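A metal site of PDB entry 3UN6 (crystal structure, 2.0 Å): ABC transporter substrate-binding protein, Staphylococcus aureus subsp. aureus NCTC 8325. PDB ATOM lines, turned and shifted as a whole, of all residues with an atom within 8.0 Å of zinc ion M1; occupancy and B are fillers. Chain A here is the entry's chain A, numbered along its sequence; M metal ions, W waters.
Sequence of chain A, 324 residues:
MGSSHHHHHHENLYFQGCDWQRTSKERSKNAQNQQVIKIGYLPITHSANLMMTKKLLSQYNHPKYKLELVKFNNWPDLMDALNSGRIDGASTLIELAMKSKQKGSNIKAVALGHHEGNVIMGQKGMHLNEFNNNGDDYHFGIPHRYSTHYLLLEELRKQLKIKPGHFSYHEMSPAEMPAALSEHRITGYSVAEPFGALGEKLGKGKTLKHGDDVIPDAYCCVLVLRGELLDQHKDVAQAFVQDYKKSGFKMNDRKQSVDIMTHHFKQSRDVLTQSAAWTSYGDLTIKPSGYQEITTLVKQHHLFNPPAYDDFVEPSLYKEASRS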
ATOM      1  N   ILE A  44     -11.875  -8.863  -0.867  1.00  0.00           N
ATOM      2  CA  ILE A  44     -12.556  -8.692   0.391  1.00  0.00           C
ATOM      3  C   ILE A  44     -11.487  -8.852   1.463  1.00  0.00           C
ATOM      4  O   ILE A  44     -10.419  -9.390   1.194  1.00  0.00           O
ATOM      5  CB  ILE A  44     -13.612  -9.752   0.576  1.00  0.00           C
ATOM      6  CG1 ILE A  44     -12.992 -11.156   0.398  1.00  0.00           C
ATOM      7  CG2 ILE A  44     -14.765  -9.514  -0.426  1.00  0.00           C
ATOM      8  CD1 ILE A  44     -13.970 -12.305   0.580  1.00  0.00           C
ATOM      9  N   THR A  45     -11.754  -8.371   2.677  1.00  0.00           N
ATOM     10  CA  THR A  45     -10.765  -8.473   3.766  1.00  0.00           C
ATOM     11  C   THR A  45     -10.400  -9.916   4.106  1.00  0.00           C
ATOM     12  O   THR A  45      -9.325 -10.176   4.651  1.00  0.00           O
ATOM     13  CB  THR A  45     -11.237  -7.815   5.074  1.00  0.00           C
ATOM     14  OG1 THR A  45     -12.337  -8.540   5.622  1.00  0.00           O
ATOM     15  CG2 THR A  45     -11.606  -6.340   4.854  1.00  0.00           C
ATOM     16  N   HIS A  46     -11.276 -10.848   3.755  1.00  0.00           N
ATOM     17  CA  HIS A  46     -11.010 -12.229   4.066  1.00  0.00           C
ATOM     18  C   HIS A  46      -9.866 -12.832   3.283  1.00  0.00           C
ATOM     19  O   HIS A  46      -9.365 -13.897   3.655  1.00  0.00           O
ATOM     20  CB  HIS A  46     -12.261 -13.101   3.912  1.00  0.00           C
ATOM     21  CG  HIS A  46     -13.394 -12.654   4.778  1.00  0.00           C
ATOM     22  ND1 HIS A  46     -14.637 -13.252   4.735  1.00  0.00           N
ATOM     23  CD2 HIS A  46     -13.499 -11.634   5.662  1.00  0.00           C
ATOM     24  CE1 HIS A  46     -15.432 -12.643   5.589  1.00  0.00           C
ATOM     25  NE2 HIS A  46     -14.769 -11.656   6.160  1.00  0.00           N
ATOM     26  N   SER A  47      -9.445 -12.149   2.228  1.00  0.00           N
ATOM     27  CA  SER A  47      -8.352 -12.639   1.414  1.00  0.00           C
ATOM     28  C   SER A  47      -7.107 -11.786   1.509  1.00  0.00           C
ATOM     29  O   SER A  47      -6.127 -12.068   0.826  1.00  0.00           O
ATOM     30  CB  SER A  47      -8.801 -12.695  -0.069  1.00  0.00           C
ATOM     31  OG  SER A  47      -8.854 -11.390  -0.609  1.00  0.00           O
ATOM     32  N   TRP A  75     -18.048 -15.888  -6.661  1.00  0.00           N
ATOM     33  CA  TRP A  75     -17.631 -17.200  -6.180  1.00  0.00           C
ATOM     34  C   TRP A  75     -17.687 -18.359  -7.184  1.00  0.00           C
ATOM     35  O   TRP A  75     -16.751 -19.167  -7.231  1.00  0.00           O
ATOM     36  CB  TRP A  75     -18.351 -17.553  -4.894  1.00  0.00           C
ATOM     37  CG  TRP A  75     -17.987 -16.627  -3.781  1.00  0.00           C
ATOM     38  CD1 TRP A  75     -18.788 -15.688  -3.212  1.00  0.00           C
ATOM     39  CD2 TRP A  75     -16.730 -16.548  -3.115  1.00  0.00           C
ATOM     40  NE1 TRP A  75     -18.111 -15.024  -2.226  1.00  0.00           N
ATOM     41  CE2 TRP A  75     -16.843 -15.537  -2.143  1.00  0.00           C
ATOM     42  CE3 TRP A  75     -15.520 -17.232  -3.240  1.00  0.00           C
ATOM     43  CZ2 TRP A  75     -15.804 -15.207  -1.294  1.00  0.00           C
ATOM     44  CZ3 TRP A  75     -14.488 -16.901  -2.419  1.00  0.00           C
ATOM     45  CH2 TRP A  75     -14.622 -15.885  -1.448  1.00  0.00           C
ATOM     46  N   SER A  91      -8.381 -18.437  -1.665  1.00  0.00           N
ATOM     47  CA  SER A  91      -9.035 -18.036  -0.408  1.00  0.00           C
ATOM     48  C   SER A  91     -10.516 -18.139  -0.782  1.00  0.00           C
ATOM     49  O   SER A  91     -10.954 -17.494  -1.739  1.00  0.00           O
ATOM     50  CB  SER A  91      -8.663 -16.605   0.004  1.00  0.00           C
ATOM     51  OG  SER A  91      -9.257 -16.289   1.248  1.00  0.00           O
ATOM     52  N   THR A  92     -11.290 -18.937  -0.052  1.00  0.00           N
ATOM     53  CA  THR A  92     -12.680 -19.214  -0.447  1.00  0.00           C
ATOM     54  C   THR A  92     -13.609 -19.510   0.714  1.00  0.00           C
ATOM     55  O   THR A  92     -13.177 -19.827   1.825  1.00  0.00           O
ATOM     56  CB  THR A  92     -12.707 -20.419  -1.476  1.00  0.00           C
ATOM     57  OG1 THR A  92     -14.018 -20.558  -2.073  1.00  0.00           O
ATOM     58  CG2 THR A  92     -12.317 -21.717  -0.804  1.00  0.00           C
ATOM     59  N   LEU A  93     -14.903 -19.378   0.452  1.00  0.00           N
ATOM     60  CA  LEU A  93     -15.925 -19.683   1.446  1.00  0.00           C
ATOM     61  C   LEU A  93     -15.723 -21.143   1.915  1.00  0.00           C
ATOM     62  O   LEU A  93     -15.589 -22.058   1.082  1.00  0.00           O
ATOM     63  CB  LEU A  93     -17.316 -19.539   0.852  1.00  0.00           C
ATOM     64  CG  LEU A  93     -17.652 -18.161   0.258  1.00  0.00           C
ATOM     65  CD1 LEU A  93     -19.023 -18.256  -0.378  1.00  0.00           C
ATOM     66  CD2 LEU A  93     -17.568 -17.061   1.332  1.00  0.00           C
ATOM     67  N   ILE A  94     -15.704 -21.361   3.221  1.00  0.00           N
ATOM     68  CA  ILE A  94     -15.428 -22.695   3.752  1.00  0.00           C
ATOM     69  C   ILE A  94     -16.535 -23.699   3.406  1.00  0.00           C
ATOM     70  O   ILE A  94     -16.237 -24.858   3.144  1.00  0.00           O
ATOM     71  CB  ILE A  94     -15.085 -22.668   5.305  1.00  0.00           C
ATOM     72  CG1 ILE A  94     -14.542 -24.018   5.758  1.00  0.00           C
ATOM     73  CG2 ILE A  94     -16.298 -22.213   6.148  1.00  0.00           C
ATOM     74  CD1 ILE A  94     -14.227 -24.107   7.273  1.00  0.00           C
ATOM     75  N   GLU A  95     -17.800 -23.248   3.355  1.00  0.00           N
ATOM     76  CA  GLU A  95     -18.916 -24.148   3.083  1.00  0.00           C
ATOM     77  C   GLU A  95     -18.896 -24.562   1.631  1.00  0.00           C
ATOM     78  O   GLU A  95     -19.196 -25.703   1.329  1.00  0.00           O
ATOM     79  CB  GLU A  95     -20.290 -23.522   3.423  1.00  0.00           C
ATOM     80  CG  GLU A  95     -20.540 -23.212   4.943  1.00  0.00           C
ATOM     81  CD  GLU A  95     -19.928 -21.895   5.446  1.00  0.00           C
ATOM     82  OE1 GLU A  95     -19.268 -21.174   4.661  1.00  0.00           O
ATOM     83  OE2 GLU A  95     -20.134 -21.561   6.641  1.00  0.00           O
ATOM     84  N   GLY A 113      -8.446 -17.658   6.426  1.00  0.00           N
ATOM     85  CA  GLY A 113      -8.031 -16.424   5.789  1.00  0.00           C
ATOM     86  C   GLY A 113      -8.055 -15.249   6.793  1.00  0.00           C
ATOM     87  O   GLY A 113      -7.347 -14.266   6.627  1.00  0.00           O
ATOM     88  N   HIS A 114      -8.834 -15.392   7.858  1.00  0.00           N
ATOM     89  CA  HIS A 114      -9.078 -14.301   8.782  1.00  0.00           C
ATOM     90  C   HIS A 114     -10.038 -14.733   9.884  1.00  0.00           C
ATOM     91  O   HIS A 114     -10.555 -15.859   9.873  1.00  0.00           O
ATOM     92  CB  HIS A 114      -9.871 -13.262   7.994  1.00  0.00           C
ATOM     93  CG  HIS A 114     -11.197 -13.819   7.587  1.00  0.00           C
ATOM     94  ND1 HIS A 114     -12.362 -13.507   8.255  1.00  0.00           N
ATOM     95  CD2 HIS A 114     -11.506 -14.800   6.719  1.00  0.00           C
ATOM     96  CE1 HIS A 114     -13.349 -14.219   7.734  1.00  0.00           C
ATOM     97  NE2 HIS A 114     -12.853 -15.018   6.815  1.00  0.00           N
ATOM     98  N   GLU A 116     -13.571 -13.031  11.822  1.00  0.00           N
ATOM     99  CA  GLU A 116     -14.594 -11.988  11.746  1.00  0.00           C
ATOM    100  C   GLU A 116     -14.674 -11.286  10.384  1.00  0.00           C
ATOM    101  O   GLU A 116     -14.582 -11.954   9.336  1.00  0.00           O
ATOM    102  CB  GLU A 116     -14.441 -10.985  12.904  1.00  0.00           C
ATOM    103  CG  GLU A 116     -14.477 -11.673  14.268  1.00  0.00           C
ATOM    104  CD  GLU A 116     -15.811 -12.396  14.592  1.00  0.00           C
ATOM    105  OE1 GLU A 116     -15.907 -12.966  15.701  1.00  0.00           O
ATOM    106  OE2 GLU A 116     -16.761 -12.377  13.765  1.00  0.00           O
ATOM    107  N   GLY A 117     -14.929  -9.981  10.387  1.00  0.00           N
ATOM    108  CA  GLY A 117     -15.008  -9.228   9.123  1.00  0.00           C
ATOM    109  C   GLY A 117     -16.281  -9.384   8.296  1.00  0.00           C
ATOM    110  O   GLY A 117     -16.311  -8.991   7.113  1.00  0.00           O
ATOM    111  N   ASN A 118     -17.334  -9.967   8.877  1.00  0.00           N
ATOM    112  CA  ASN A 118     -18.648 -10.125   8.200  1.00  0.00           C
ATOM    113  C   ASN A 118     -19.678  -9.146   8.751  1.00  0.00           C
ATOM    114  O   ASN A 118     -19.640  -8.773   9.929  1.00  0.00           O
ATOM    115  CB  ASN A 118     -19.177 -11.576   8.348  1.00  0.00           C
ATOM    116  CG  ASN A 118     -18.567 -12.532   7.315  1.00  0.00           C
ATOM    117  OD1 ASN A 118     -18.380 -12.145   6.163  1.00  0.00           O
ATOM    118  ND2 ASN A 118     -18.298 -13.791   7.706  1.00  0.00           N
ATOM    119  N   PRO A 143     -23.602 -14.037  -0.686  1.00  0.00           N
ATOM    120  CA  PRO A 143     -22.625 -14.275  -1.769  1.00  0.00           C
ATOM    121  C   PRO A 143     -22.749 -15.645  -2.476  1.00  0.00           C
ATOM    122  O   PRO A 143     -22.356 -15.785  -3.634  1.00  0.00           O
ATOM    123  CB  PRO A 143     -21.268 -14.126  -1.066  1.00  0.00           C
ATOM    124  CG  PRO A 143     -21.549 -13.685   0.317  1.00  0.00           C
ATOM    125  CD  PRO A 143     -22.964 -13.981   0.637  1.00  0.00           C
ATOM    126  N   SER A 147     -22.587 -20.545   2.367  1.00  0.00           N
ATOM    127  CA  SER A 147     -21.806 -19.481   2.949  1.00  0.00           C
ATOM    128  C   SER A 147     -22.150 -19.283   4.406  1.00  0.00           C
ATOM    129  O   SER A 147     -23.231 -19.622   4.828  1.00  0.00           O
ATOM    130  CB  SER A 147     -22.041 -18.166   2.201  1.00  0.00           C
ATOM    131  OG  SER A 147     -23.380 -17.669   2.334  1.00  0.00           O
ATOM    132  N   THR A 148     -21.180 -18.773   5.160  1.00  0.00           N
ATOM    133  CA  THR A 148     -21.381 -18.401   6.561  1.00  0.00           C
ATOM    134  C   THR A 148     -22.413 -17.265   6.654  1.00  0.00           C
ATOM    135  O   THR A 148     -23.074 -17.096   7.657  1.00  0.00           O
ATOM    136  CB  THR A 148     -20.024 -17.986   7.163  1.00  0.00           C
ATOM    137  OG1 THR A 148     -19.194 -19.140   7.224  1.00  0.00           O
ATOM    138  CG2 THR A 148     -20.154 -17.363   8.599  1.00  0.00           C
ATOM    139  N   HIS A 149     -22.540 -16.493   5.580  1.00  0.00           N
ATOM    140  CA  HIS A 149     -23.500 -15.391   5.498  1.00  0.00           C
ATOM    141  C   HIS A 149     -24.916 -15.901   5.600  1.00  0.00           C
ATOM    142  O   HIS A 149     -25.713 -15.353   6.356  1.00  0.00           O
ATOM    143  CB  HIS A 149     -23.239 -14.621   4.205  1.00  0.00           C
ATOM    144  CG  HIS A 149     -21.810 -14.257   4.046  1.00  0.00           C
ATOM    145  ND1 HIS A 149     -20.923 -15.050   3.346  1.00  0.00           N
ATOM    146  CD2 HIS A 149     -21.082 -13.253   4.593  1.00  0.00           C
ATOM    147  CE1 HIS A 149     -19.720 -14.516   3.432  1.00  0.00           C
ATOM    148  NE2 HIS A 149     -19.786 -13.421   4.179  1.00  0.00           N
ATOM    149  N   VAL A 191     -22.312 -10.010   3.935  1.00  0.00           N
ATOM    150  CA  VAL A 191     -21.139 -10.180   3.106  1.00  0.00           C
ATOM    151  C   VAL A 191     -19.899  -9.791   3.876  1.00  0.00           C
ATOM    152  O   VAL A 191     -19.989  -9.267   4.987  1.00  0.00           O
ATOM    153  CB  VAL A 191     -21.257  -9.265   1.870  1.00  0.00           C
ATOM    154  CG1 VAL A 191     -21.214  -7.773   2.320  1.00  0.00           C
ATOM    155  CG2 VAL A 191     -20.167  -9.579   0.848  1.00  0.00           C
ATOM    156  N   ALA A 192     -18.729 -10.115   3.316  1.00  0.00           N
ATOM    157  CA  ALA A 192     -17.471  -9.729   3.935  1.00  0.00           C
ATOM    158  C   ALA A 192     -17.233  -8.264   3.644  1.00  0.00           C
ATOM    159  O   ALA A 192     -17.661  -7.743   2.603  1.00  0.00           O
ATOM    160  CB  ALA A 192     -16.306 -10.553   3.373  1.00  0.00           C
ATOM    161  N   GLU A 193     -16.542  -7.582   4.533  1.00  0.00           N
ATOM    162  CA  GLU A 193     -16.137  -6.215   4.243  1.00  0.00           C
ATOM    163  C   GLU A 193     -15.164  -6.348   3.066  1.00  0.00           C
ATOM    164  O   GLU A 193     -14.577  -7.407   2.874  1.00  0.00           O
ATOM    165  CB  GLU A 193     -15.516  -5.560   5.441  1.00  0.00           C
ATOM    166  CG  GLU A 193     -16.516  -5.267   6.563  1.00  0.00           C
ATOM    167  CD  GLU A 193     -17.558  -4.177   6.216  1.00  0.00           C
ATOM    168  OE1 GLU A 193     -17.904  -3.991   5.029  1.00  0.00           O
ATOM    169  OE2 GLU A 193     -18.061  -3.510   7.159  1.00  0.00           O
ATOM    170  N   ALA A 218     -17.356 -17.090  13.876  1.00  0.00           N
ATOM    171  CA  ALA A 218     -17.772 -18.067  12.889  1.00  0.00           C
ATOM    172  C   ALA A 218     -16.731 -18.083  11.782  1.00  0.00           C
ATOM    173  O   ALA A 218     -16.355 -17.035  11.260  1.00  0.00           O
ATOM    174  CB  ALA A 218     -19.134 -17.683  12.317  1.00  0.00           C
ATOM    175  N   TYR A 219     -16.253 -19.249  11.414  1.00  0.00           N
ATOM    176  CA  TYR A 219     -15.314 -19.304  10.324  1.00  0.00           C
ATOM    177  C   TYR A 219     -16.036 -18.922   9.028  1.00  0.00           C
ATOM    178  O   TYR A 219     -17.236 -19.232   8.860  1.00  0.00           O
ATOM    179  CB  TYR A 219     -14.668 -20.683  10.192  1.00  0.00           C
ATOM    180  CG  TYR A 219     -13.751 -21.107  11.302  1.00  0.00           C
ATOM    181  CD1 TYR A 219     -13.210 -20.187  12.215  1.00  0.00           C
ATOM    182  CD2 TYR A 219     -13.305 -22.423  11.372  1.00  0.00           C
ATOM    183  CE1 TYR A 219     -12.330 -20.601  13.211  1.00  0.00           C
ATOM    184  CE2 TYR A 219     -12.410 -22.840  12.342  1.00  0.00           C
ATOM    185  CZ  TYR A 219     -11.920 -21.920  13.262  1.00  0.00           C
ATOM    186  OH  TYR A 219     -11.031 -22.346  14.218  1.00  0.00           O
ATOM    187  N   CYS A 220     -15.333 -18.220   8.143  1.00  0.00           N
ATOM    188  CA  CYS A 220     -15.890 -17.834   6.849  1.00  0.00           C
ATOM    189  C   CYS A 220     -14.995 -18.319   5.691  1.00  0.00           C
ATOM    190  O   CYS A 220     -15.308 -19.280   5.037  1.00  0.00           O
ATOM    191  CB  CYS A 220     -16.131 -16.337   6.780  1.00  0.00           C
ATOM    192  SG  CYS A 220     -17.011 -15.837   5.255  1.00  0.00           S
ATOM    193  N   CYS A 221     -13.898 -17.636   5.434  1.00  0.00           N
ATOM    194  CA  CYS A 221     -13.021 -18.035   4.359  1.00  0.00           C
ATOM    195  C   CYS A 221     -11.789 -18.789   4.832  1.00  0.00           C
ATOM    196  O   CYS A 221     -11.224 -18.490   5.889  1.00  0.00           O
ATOM    197  CB  CYS A 221     -12.592 -16.834   3.526  1.00  0.00           C
ATOM    198  SG  CYS A 221     -13.921 -16.136   2.475  1.00  0.00           S
ATOM    199  N   VAL A 222     -11.342 -19.721   4.004  1.00  0.00           N
ATOM    200  CA  VAL A 222     -10.139 -20.539   4.282  1.00  0.00           C
ATOM    201  C   VAL A 222      -9.227 -20.546   3.055  1.00  0.00           C
ATOM    202  O   VAL A 222      -9.674 -20.348   1.925  1.00  0.00           O
ATOM    203  CB  VAL A 222     -10.511 -22.046   4.583  1.00  0.00           C
ATOM    204  CG1 VAL A 222     -11.071 -22.199   5.993  1.00  0.00           C
ATOM    205  CG2 VAL A 222     -11.458 -22.579   3.522  1.00  0.00           C
HETATM  206 ZN    ZN M   1     -15.400 -14.941   3.728  1.00  0.00          ZN
HETATM  207 ZN    ZN M   2     -17.937 -12.573   0.587  1.00  0.00          ZN
HETATM  208  O   HOH W   1     -16.818 -13.883   2.123  1.00  0.00           O
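Leu 93 touches zinc ion M1 (CD2 to ZN, 3.9 Å). Four residues have an atom within 4 Å of zinc ion M1: His 46, Leu 93, Cys 220 and Cys 221.
Zinc ion M1 is bound by a ring nitrogen (ND1) of His 46 (2.1 Å), the side-chain sulfur of Cys 221 (2.3 Å), water W1 (2.4 Å) and the side-chain sulfur of Cys 220 (2.4 Å). Zinc ion M1 has four donor atoms within binding distance.
A ring nitrogen (NE2) of His 114 lies close to a ring nitrogen (ND1) of His 46 (3.3 Å). A ring nitrogen (NE2) of His 46 is in hydrogen-bond range of the backbone carbonyl oxygen (O) of Glu 116. O of His 46 sits at hydrogen-bond distance from OG of Ser 91 (3.4 Å). The backbone carbonyl oxygen (O) of Gly 117 is in hydrogen-bond range of a ring nitrogen (NE2) of His 46, 3.2 Å away. The backbone NH (N) of Cys 221 lies within hydrogen-bond range of a ring nitrogen (NE2) of His 114, 3.1 Å away. The backbone carbonyl oxygen (O) of Cys 221 is in hydrogen-bond range of the backbone NH (N) of Gly 113 (2.9 Å). SG of Cys 220 lies close to ND2 of Asn 118 (3.4 Å). O of Cys 220 is in hydrogen-bond range of N of Ile 94, at 2.8 Å.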
